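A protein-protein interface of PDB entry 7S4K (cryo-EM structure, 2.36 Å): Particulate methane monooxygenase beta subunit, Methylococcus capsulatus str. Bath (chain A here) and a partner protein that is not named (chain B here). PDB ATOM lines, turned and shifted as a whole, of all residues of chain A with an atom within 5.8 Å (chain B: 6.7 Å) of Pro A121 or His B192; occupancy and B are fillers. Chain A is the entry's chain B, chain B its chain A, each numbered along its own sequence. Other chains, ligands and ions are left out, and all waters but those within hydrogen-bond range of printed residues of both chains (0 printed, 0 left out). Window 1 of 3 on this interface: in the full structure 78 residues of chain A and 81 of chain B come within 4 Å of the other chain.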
ATOM      1  N   ASP A  49      18.864  20.095 -15.498  1.00  0.00           N
ATOM      2  CA  ASP A  49      19.176  21.019 -14.421  1.00  0.00           C
ATOM      3  C   ASP A  49      17.961  21.783 -13.922  1.00  0.00           C
ATOM      4  O   ASP A  49      18.031  22.390 -12.850  1.00  0.00           O
ATOM      5  CB  ASP A  49      20.242  22.013 -14.881  1.00  0.00           C
ATOM      6  CG  ASP A  49      21.050  22.563 -13.731  1.00  0.00           C
ATOM      7  OD1 ASP A  49      21.651  21.761 -12.989  1.00  0.00           O
ATOM      8  OD2 ASP A  49      21.085  23.798 -13.568  1.00  0.00           O
ATOM      9  N   LYS A  55      16.350  14.938 -12.498  1.00  0.00           N
ATOM     10  CA  LYS A  55      17.649  14.542 -11.945  1.00  0.00           C
ATOM     11  C   LYS A  55      17.640  13.044 -11.631  1.00  0.00           C
ATOM     12  O   LYS A  55      17.358  12.608 -10.513  1.00  0.00           O
ATOM     13  CB  LYS A  55      17.976  15.353 -10.699  1.00  0.00           C
ATOM     14  CG  LYS A  55      17.701  16.834 -10.817  1.00  0.00           C
ATOM     15  CD  LYS A  55      18.971  17.614 -11.041  1.00  0.00           C
ATOM     16  CE  LYS A  55      18.845  19.033 -10.538  1.00  0.00           C
ATOM     17  NZ  LYS A  55      17.826  19.791 -11.301  1.00  0.00           N
ATOM     18  N   LEU A  97      26.868  28.585 -11.726  1.00  0.00           N
ATOM     19  CA  LEU A  97      25.995  28.418 -10.570  1.00  0.00           C
ATOM     20  C   LEU A  97      25.329  29.728 -10.182  1.00  0.00           C
ATOM     21  O   LEU A  97      24.145  29.747  -9.842  1.00  0.00           O
ATOM     22  CB  LEU A  97      26.785  27.854  -9.394  1.00  0.00           C
ATOM     23  CG  LEU A  97      27.032  26.350  -9.451  1.00  0.00           C
ATOM     24  CD1 LEU A  97      28.103  25.951  -8.457  1.00  0.00           C
ATOM     25  CD2 LEU A  97      25.744  25.601  -9.188  1.00  0.00           C
ATOM     26  N   GLU A 100      22.643  30.545 -12.845  1.00  0.00           N
ATOM     27  CA  GLU A 100      21.513  29.594 -12.677  1.00  0.00           C
ATOM     28  C   GLU A 100      20.705  29.989 -11.445  1.00  0.00           C
ATOM     29  O   GLU A 100      19.487  30.124 -11.582  1.00  0.00           O
ATOM     30  CB  GLU A 100      22.013  28.165 -12.486  1.00  0.00           C
ATOM     31  CG  GLU A 100      22.242  27.419 -13.784  1.00  0.00           C
ATOM     32  CD  GLU A 100      23.196  26.242 -13.674  1.00  0.00           C
ATOM     33  OE1 GLU A 100      23.819  26.075 -12.605  1.00  0.00           O
ATOM     34  OE2 GLU A 100      23.318  25.495 -14.662  1.00  0.00           O
ATOM     35  N   TRP A 101      21.367  30.196 -10.303  1.00  0.00           N
ATOM     36  CA  TRP A 101      20.645  30.473  -9.067  1.00  0.00           C
ATOM     37  C   TRP A 101      19.887  31.788  -9.139  1.00  0.00           C
ATOM     38  O   TRP A 101      18.765  31.882  -8.629  1.00  0.00           O
ATOM     39  CB  TRP A 101      21.609  30.482  -7.884  1.00  0.00           C
ATOM     40  CG  TRP A 101      21.642  29.189  -7.145  1.00  0.00           C
ATOM     41  CD1 TRP A 101      22.687  28.321  -7.064  1.00  0.00           C
ATOM     42  CD2 TRP A 101      20.578  28.607  -6.386  1.00  0.00           C
ATOM     43  NE1 TRP A 101      22.342  27.237  -6.299  1.00  0.00           N
ATOM     44  CE2 TRP A 101      21.051  27.389  -5.871  1.00  0.00           C
ATOM     45  CE3 TRP A 101      19.270  29.001  -6.091  1.00  0.00           C
ATOM     46  CZ2 TRP A 101      20.265  26.560  -5.077  1.00  0.00           C
ATOM     47  CZ3 TRP A 101      18.494  28.178  -5.306  1.00  0.00           C
ATOM     48  CH2 TRP A 101      18.992  26.971  -4.807  1.00  0.00           C
ATOM     49  N   ARG A 104      16.850  30.966 -11.127  1.00  0.00           N
ATOM     50  CA  ARG A 104      15.931  30.112 -10.382  1.00  0.00           C
ATOM     51  C   ARG A 104      15.156  30.916  -9.353  1.00  0.00           C
ATOM     52  O   ARG A 104      13.939  30.756  -9.218  1.00  0.00           O
ATOM     53  CB  ARG A 104      16.688  28.988  -9.675  1.00  0.00           C
ATOM     54  CG  ARG A 104      17.370  27.957 -10.550  1.00  0.00           C
ATOM     55  CD  ARG A 104      16.666  27.706 -11.857  1.00  0.00           C
ATOM     56  NE  ARG A 104      17.617  27.307 -12.886  1.00  0.00           N
ATOM     57  CZ  ARG A 104      18.094  26.080 -13.030  1.00  0.00           C
ATOM     58  NH1 ARG A 104      17.735  25.098 -12.222  1.00  0.00           N
ATOM     59  NH2 ARG A 104      18.959  25.831 -14.007  1.00  0.00           N
ATOM     60  N   VAL A 119      13.057  23.349  -8.365  1.00  0.00           N
ATOM     61  CA  VAL A 119      13.816  23.884  -9.491  1.00  0.00           C
ATOM     62  C   VAL A 119      15.260  24.221  -9.112  1.00  0.00           C
ATOM     63  O   VAL A 119      15.885  25.052  -9.763  1.00  0.00           O
ATOM     64  CB  VAL A 119      13.115  25.102 -10.112  1.00  0.00           C
ATOM     65  CG1 VAL A 119      11.763  24.707 -10.667  1.00  0.00           C
ATOM     66  CG2 VAL A 119      12.978  26.218  -9.092  1.00  0.00           C
ATOM     67  N   PHE A 120      15.808  23.587  -8.081  1.00  0.00           N
ATOM     68  CA  PHE A 120      17.197  23.836  -7.722  1.00  0.00           C
ATOM     69  C   PHE A 120      18.144  23.315  -8.805  1.00  0.00           C
ATOM     70  O   PHE A 120      17.828  22.353  -9.508  1.00  0.00           O
ATOM     71  CB  PHE A 120      17.531  23.175  -6.389  1.00  0.00           C
ATOM     72  CG  PHE A 120      17.433  21.680  -6.417  1.00  0.00           C
ATOM     73  CD1 PHE A 120      16.233  21.051  -6.152  1.00  0.00           C
ATOM     74  CD2 PHE A 120      18.537  20.903  -6.712  1.00  0.00           C
ATOM     75  CE1 PHE A 120      16.138  19.682  -6.181  1.00  0.00           C
ATOM     76  CE2 PHE A 120      18.445  19.532  -6.745  1.00  0.00           C
ATOM     77  CZ  PHE A 120      17.244  18.921  -6.477  1.00  0.00           C
ATOM     78  N   PRO A 121      19.310  23.931  -8.959  1.00  0.00           N
ATOM     79  CA  PRO A 121      20.299  23.452  -9.929  1.00  0.00           C
ATOM     80  C   PRO A 121      21.228  22.413  -9.307  1.00  0.00           C
ATOM     81  O   PRO A 121      21.197  22.144  -8.110  1.00  0.00           O
ATOM     82  CB  PRO A 121      21.055  24.725 -10.300  1.00  0.00           C
ATOM     83  CG  PRO A 121      20.999  25.544  -9.069  1.00  0.00           C
ATOM     84  CD  PRO A 121      19.684  25.242  -8.400  1.00  0.00           C
ATOM     85  N   ALA A 122      22.076  21.835 -10.152  1.00  0.00           N
ATOM     86  CA  ALA A 122      23.027  20.821  -9.727  1.00  0.00           C
ATOM     87  C   ALA A 122      24.296  21.464  -9.185  1.00  0.00           C
ATOM     88  O   ALA A 122      24.610  22.617  -9.487  1.00  0.00           O
ATOM     89  CB  ALA A 122      23.377  19.886 -10.885  1.00  0.00           C
ATOM     90  N   SER A 123      25.029  20.700  -8.380  1.00  0.00           N
ATOM     91  CA  SER A 123      26.262  21.171  -7.766  1.00  0.00           C
ATOM     92  C   SER A 123      27.461  20.661  -8.557  1.00  0.00           C
ATOM     93  O   SER A 123      27.527  19.478  -8.900  1.00  0.00           O
ATOM     94  CB  SER A 123      26.342  20.707  -6.312  1.00  0.00           C
ATOM     95  OG  SER A 123      27.499  21.213  -5.676  1.00  0.00           O
ATOM     96  N   ASN A 160      26.173  15.626  -5.614  1.00  0.00           N
ATOM     97  CA  ASN A 160      24.786  16.060  -5.594  1.00  0.00           C
ATOM     98  C   ASN A 160      23.883  15.159  -4.766  1.00  0.00           C
ATOM     99  O   ASN A 160      22.724  15.516  -4.542  1.00  0.00           O
ATOM    100  CB  ASN A 160      24.236  16.135  -7.018  1.00  0.00           C
ATOM    101  CG  ASN A 160      24.792  17.302  -7.791  1.00  0.00           C
ATOM    102  OD1 ASN A 160      24.261  18.406  -7.729  1.00  0.00           O
ATOM    103  ND2 ASN A 160      25.860  17.063  -8.537  1.00  0.00           N
ATOM    104  N   ILE A 163      21.869  16.500  -1.723  1.00  0.00           N
ATOM    105  CA  ILE A 163      20.750  17.375  -2.053  1.00  0.00           C
ATOM    106  C   ILE A 163      19.548  16.569  -2.523  1.00  0.00           C
ATOM    107  O   ILE A 163      18.426  16.765  -2.045  1.00  0.00           O
ATOM    108  CB  ILE A 163      21.178  18.410  -3.108  1.00  0.00           C
ATOM    109  CG1 ILE A 163      22.301  19.289  -2.567  1.00  0.00           C
ATOM    110  CG2 ILE A 163      19.997  19.259  -3.528  1.00  0.00           C
ATOM    111  CD1 ILE A 163      23.223  19.814  -3.633  1.00  0.00           C
ATOM    112  N   ASN B 187      18.016  22.199   3.241  1.00  0.00           N
ATOM    113  CA  ASN B 187      19.162  21.353   2.921  1.00  0.00           C
ATOM    114  C   ASN B 187      19.772  21.731   1.578  1.00  0.00           C
ATOM    115  O   ASN B 187      21.002  21.817   1.445  1.00  0.00           O
ATOM    116  CB  ASN B 187      18.730  19.889   2.930  1.00  0.00           C
ATOM    117  CG  ASN B 187      19.832  18.956   2.499  1.00  0.00           C
ATOM    118  OD1 ASN B 187      20.850  18.831   3.174  1.00  0.00           O
ATOM    119  ND2 ASN B 187      19.634  18.287   1.372  1.00  0.00           N
ATOM    120  N   THR B 188      18.928  21.963   0.569  1.00  0.00           N
ATOM    121  CA  THR B 188      19.433  22.376  -0.735  1.00  0.00           C
ATOM    122  C   THR B 188      20.192  23.692  -0.638  1.00  0.00           C
ATOM    123  O   THR B 188      21.304  23.822  -1.174  1.00  0.00           O
ATOM    124  CB  THR B 188      18.278  22.509  -1.723  1.00  0.00           C
ATOM    125  OG1 THR B 188      17.577  21.265  -1.813  1.00  0.00           O
ATOM    126  CG2 THR B 188      18.799  22.886  -3.089  1.00  0.00           C
ATOM    127  N   TYR B 189      19.606  24.672   0.053  1.00  0.00           N
ATOM    128  CA  TYR B 189      20.260  25.963   0.221  1.00  0.00           C
ATOM    129  C   TYR B 189      21.599  25.801   0.920  1.00  0.00           C
ATOM    130  O   TYR B 189      22.605  26.381   0.500  1.00  0.00           O
ATOM    131  CB  TYR B 189      19.360  26.908   1.013  1.00  0.00           C
ATOM    132  CG  TYR B 189      18.344  27.642   0.179  1.00  0.00           C
ATOM    133  CD1 TYR B 189      18.657  28.096  -1.092  1.00  0.00           C
ATOM    134  CD2 TYR B 189      17.071  27.888   0.666  1.00  0.00           C
ATOM    135  CE1 TYR B 189      17.731  28.772  -1.854  1.00  0.00           C
ATOM    136  CE2 TYR B 189      16.138  28.560  -0.090  1.00  0.00           C
ATOM    137  CZ  TYR B 189      16.472  29.001  -1.347  1.00  0.00           C
ATOM    138  OH  TYR B 189      15.543  29.674  -2.104  1.00  0.00           O
ATOM    139  N   PHE B 190      21.631  25.004   1.989  1.00  0.00           N
ATOM    140  CA  PHE B 190      22.859  24.833   2.750  1.00  0.00           C
ATOM    141  C   PHE B 190      23.960  24.236   1.890  1.00  0.00           C
ATOM    142  O   PHE B 190      25.092  24.726   1.884  1.00  0.00           O
ATOM    143  CB  PHE B 190      22.617  23.951   3.973  1.00  0.00           C
ATOM    144  CG  PHE B 190      23.881  23.423   4.581  1.00  0.00           C
ATOM    145  CD1 PHE B 190      24.647  24.220   5.413  1.00  0.00           C
ATOM    146  CD2 PHE B 190      24.319  22.140   4.304  1.00  0.00           C
ATOM    147  CE1 PHE B 190      25.814  23.745   5.964  1.00  0.00           C
ATOM    148  CE2 PHE B 190      25.488  21.662   4.852  1.00  0.00           C
ATOM    149  CZ  PHE B 190      26.235  22.465   5.685  1.00  0.00           C
ATOM    150  N   TRP B 191      23.652  23.158   1.169  1.00  0.00           N
ATOM    151  CA  TRP B 191      24.703  22.490   0.408  1.00  0.00           C
ATOM    152  C   TRP B 191      25.207  23.363  -0.732  1.00  0.00           C
ATOM    153  O   TRP B 191      26.421  23.450  -0.968  1.00  0.00           O
ATOM    154  CB  TRP B 191      24.210  21.141  -0.107  1.00  0.00           C
ATOM    155  CG  TRP B 191      24.342  20.075   0.924  1.00  0.00           C
ATOM    156  CD1 TRP B 191      23.338  19.351   1.484  1.00  0.00           C
ATOM    157  CD2 TRP B 191      25.554  19.627   1.538  1.00  0.00           C
ATOM    158  NE1 TRP B 191      23.846  18.474   2.407  1.00  0.00           N
ATOM    159  CE2 TRP B 191      25.206  18.623   2.458  1.00  0.00           C
ATOM    160  CE3 TRP B 191      26.900  19.973   1.396  1.00  0.00           C
ATOM    161  CZ2 TRP B 191      26.152  17.961   3.231  1.00  0.00           C
ATOM    162  CZ3 TRP B 191      27.836  19.317   2.164  1.00  0.00           C
ATOM    163  CH2 TRP B 191      27.460  18.323   3.071  1.00  0.00           C
ATOM    164  N   HIS B 192      24.296  24.033  -1.442  1.00  0.00           N
ATOM    165  CA  HIS B 192      24.744  24.897  -2.525  1.00  0.00           C
ATOM    166  C   HIS B 192      25.564  26.067  -1.996  1.00  0.00           C
ATOM    167  O   HIS B 192      26.597  26.416  -2.577  1.00  0.00           O
ATOM    168  CB  HIS B 192      23.551  25.381  -3.340  1.00  0.00           C
ATOM    169  CG  HIS B 192      23.224  24.493  -4.497  1.00  0.00           C
ATOM    170  ND1 HIS B 192      23.929  24.525  -5.680  1.00  0.00           N
ATOM    171  CD2 HIS B 192      22.280  23.536  -4.648  1.00  0.00           C
ATOM    172  CE1 HIS B 192      23.428  23.633  -6.513  1.00  0.00           C
ATOM    173  NE2 HIS B 192      22.426  23.019  -5.912  1.00  0.00           N
ATOM    174  N   ALA B 193      25.139  26.669  -0.881  1.00  0.00           N
ATOM    175  CA  ALA B 193      25.901  27.766  -0.298  1.00  0.00           C
ATOM    176  C   ALA B 193      27.265  27.297   0.185  1.00  0.00           C
ATOM    177  O   ALA B 193      28.258  28.014   0.038  1.00  0.00           O
ATOM    178  CB  ALA B 193      25.117  28.400   0.848  1.00  0.00           C
ATOM    179  N   PHE B 194      27.334  26.099   0.763  1.00  0.00           N
ATOM    180  CA  PHE B 194      28.605  25.571   1.246  1.00  0.00           C
ATOM    181  C   PHE B 194      29.586  25.366   0.100  1.00  0.00           C
ATOM    182  O   PHE B 194      30.753  25.769   0.184  1.00  0.00           O
ATOM    183  CB  PHE B 194      28.356  24.262   1.996  1.00  0.00           C
ATOM    184  CG  PHE B 194      29.605  23.514   2.348  1.00  0.00           C
ATOM    185  CD1 PHE B 194      30.299  23.810   3.505  1.00  0.00           C
ATOM    186  CD2 PHE B 194      30.076  22.502   1.530  1.00  0.00           C
ATOM    187  CE1 PHE B 194      31.445  23.120   3.834  1.00  0.00           C
ATOM    188  CE2 PHE B 194      31.221  21.811   1.854  1.00  0.00           C
ATOM    189  CZ  PHE B 194      31.905  22.120   3.007  1.00  0.00           C
ATOM    190  N   TRP B 195      29.133  24.742  -0.988  1.00  0.00           N
ATOM    191  CA  TRP B 195      30.049  24.506  -2.100  1.00  0.00           C
ATOM    192  C   TRP B 195      30.428  25.811  -2.792  1.00  0.00           C
ATOM    193  O   TRP B 195      31.579  25.984  -3.219  1.00  0.00           O
ATOM    194  CB  TRP B 195      29.443  23.510  -3.083  1.00  0.00           C
ATOM    195  CG  TRP B 195      29.562  22.101  -2.596  1.00  0.00           C
ATOM    196  CD1 TRP B 195      28.545  21.230  -2.360  1.00  0.00           C
ATOM    197  CD2 TRP B 195      30.770  21.406  -2.263  1.00  0.00           C
ATOM    198  NE1 TRP B 195      29.040  20.034  -1.909  1.00  0.00           N
ATOM    199  CE2 TRP B 195      30.405  20.117  -1.840  1.00  0.00           C
ATOM    200  CE3 TRP B 195      32.124  21.750  -2.287  1.00  0.00           C
ATOM    201  CZ2 TRP B 195      31.343  19.170  -1.444  1.00  0.00           C
ATOM    202  CZ3 TRP B 195      33.053  20.810  -1.893  1.00  0.00           C
ATOM    203  CH2 TRP B 195      32.659  19.536  -1.478  1.00  0.00           C
ATOM    204  N   PHE B 196      29.485  26.749  -2.893  1.00  0.00           N
ATOM    205  CA  PHE B 196      29.817  28.059  -3.436  1.00  0.00           C
ATOM    206  C   PHE B 196      30.855  28.759  -2.573  1.00  0.00           C
ATOM    207  O   PHE B 196      31.779  29.391  -3.094  1.00  0.00           O
ATOM    208  CB  PHE B 196      28.555  28.909  -3.558  1.00  0.00           C
ATOM    209  CG  PHE B 196      28.645  29.970  -4.608  1.00  0.00           C
ATOM    210  CD1 PHE B 196      29.135  31.225  -4.301  1.00  0.00           C
ATOM    211  CD2 PHE B 196      28.245  29.712  -5.905  1.00  0.00           C
ATOM    212  CE1 PHE B 196      29.221  32.203  -5.267  1.00  0.00           C
ATOM    213  CE2 PHE B 196      28.328  30.686  -6.874  1.00  0.00           C
ATOM    214  CZ  PHE B 196      28.817  31.933  -6.554  1.00  0.00           C
ATOM    215  N   ALA B 197      30.723  28.655  -1.250  1.00  0.00           N
ATOM    216  CA  ALA B 197      31.697  29.265  -0.355  1.00  0.00           C
ATOM    217  C   ALA B 197      33.062  28.614  -0.501  1.00  0.00           C
ATOM    218  O   ALA B 197      34.088  29.292  -0.416  1.00  0.00           O
ATOM    219  CB  ALA B 197      31.211  29.177   1.090  1.00  0.00           C
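Of the printed residues of chain B, Trp A101 touches Tyr B189 and His B192. Of the printed residues of chain B, Ser A123 touches His B192 and Trp B195. Arg A104 touches none of the printed residues of chain B. Val A119 touches none of the printed residues of chain B. The nearest residue of chain A that does not touch His B192 is Leu A97 (4.05 Å). The nearest printed residue of chain A that does not touch Thr B188 is Trp A101 (4.4 Å).
A ring nitrogen (ND1) of His B192 is in hydrogen-bond range of the indole nitrogen (NE1) of Trp A101, 3.2 Å away. O of Pro A121 lies within hydrogen-bond range of NE2 of His B192 (2.7 Å).
NE1 of Trp B191 lies close to OD1 of Asn B187, 3.1 Å away. The backbone NH (N) of Ala A122 is in hydrogen-bond range of the side-chain carboxylate (OD1) of Asp A49 (2.9 Å). O of Phe A120 lies within hydrogen-bond range of NZ of Lys A55 (3.1 Å). The side-chain amide oxygen (OD1) of Asn A160 lies within hydrogen-bond range of the backbone NH (N) of Ser A123, at 2.5 Å.
Tyr B189 touches Trp A101 (CE1 to CZ3, 3.6 Å). Thr B188 touches Phe A120 (CG2 to CB, 3.5 Å). His B192 touches Ala A122 (CE1 to O, 3.4 Å). CE1 of His B192 touches N of Ser A123, 3.8 Å away. Ser A123 touches Trp B195 (OG to CD1, 3.5 Å). Asn B187 touches Ile A163 (ND2 to CA, 3.7 Å). OG1 of Thr B188 touches CG2 of Ile A163, 3.6 Å away. Ile A163 touches Trp B191. His B192 touches Ile A163.
Hydrophobic or aromatic side chains of chain B that line the printed part of chain A: Tyr B189, Trp B191, His B192 and Trp B195. Along chain A the printed residues that touch a printed residue of chain B span positions 101 to 163. Among the printed residues, no Asp or Glu carboxylate lies within 4 Å of a Lys or Arg side-chain nitrogen of the other chain.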
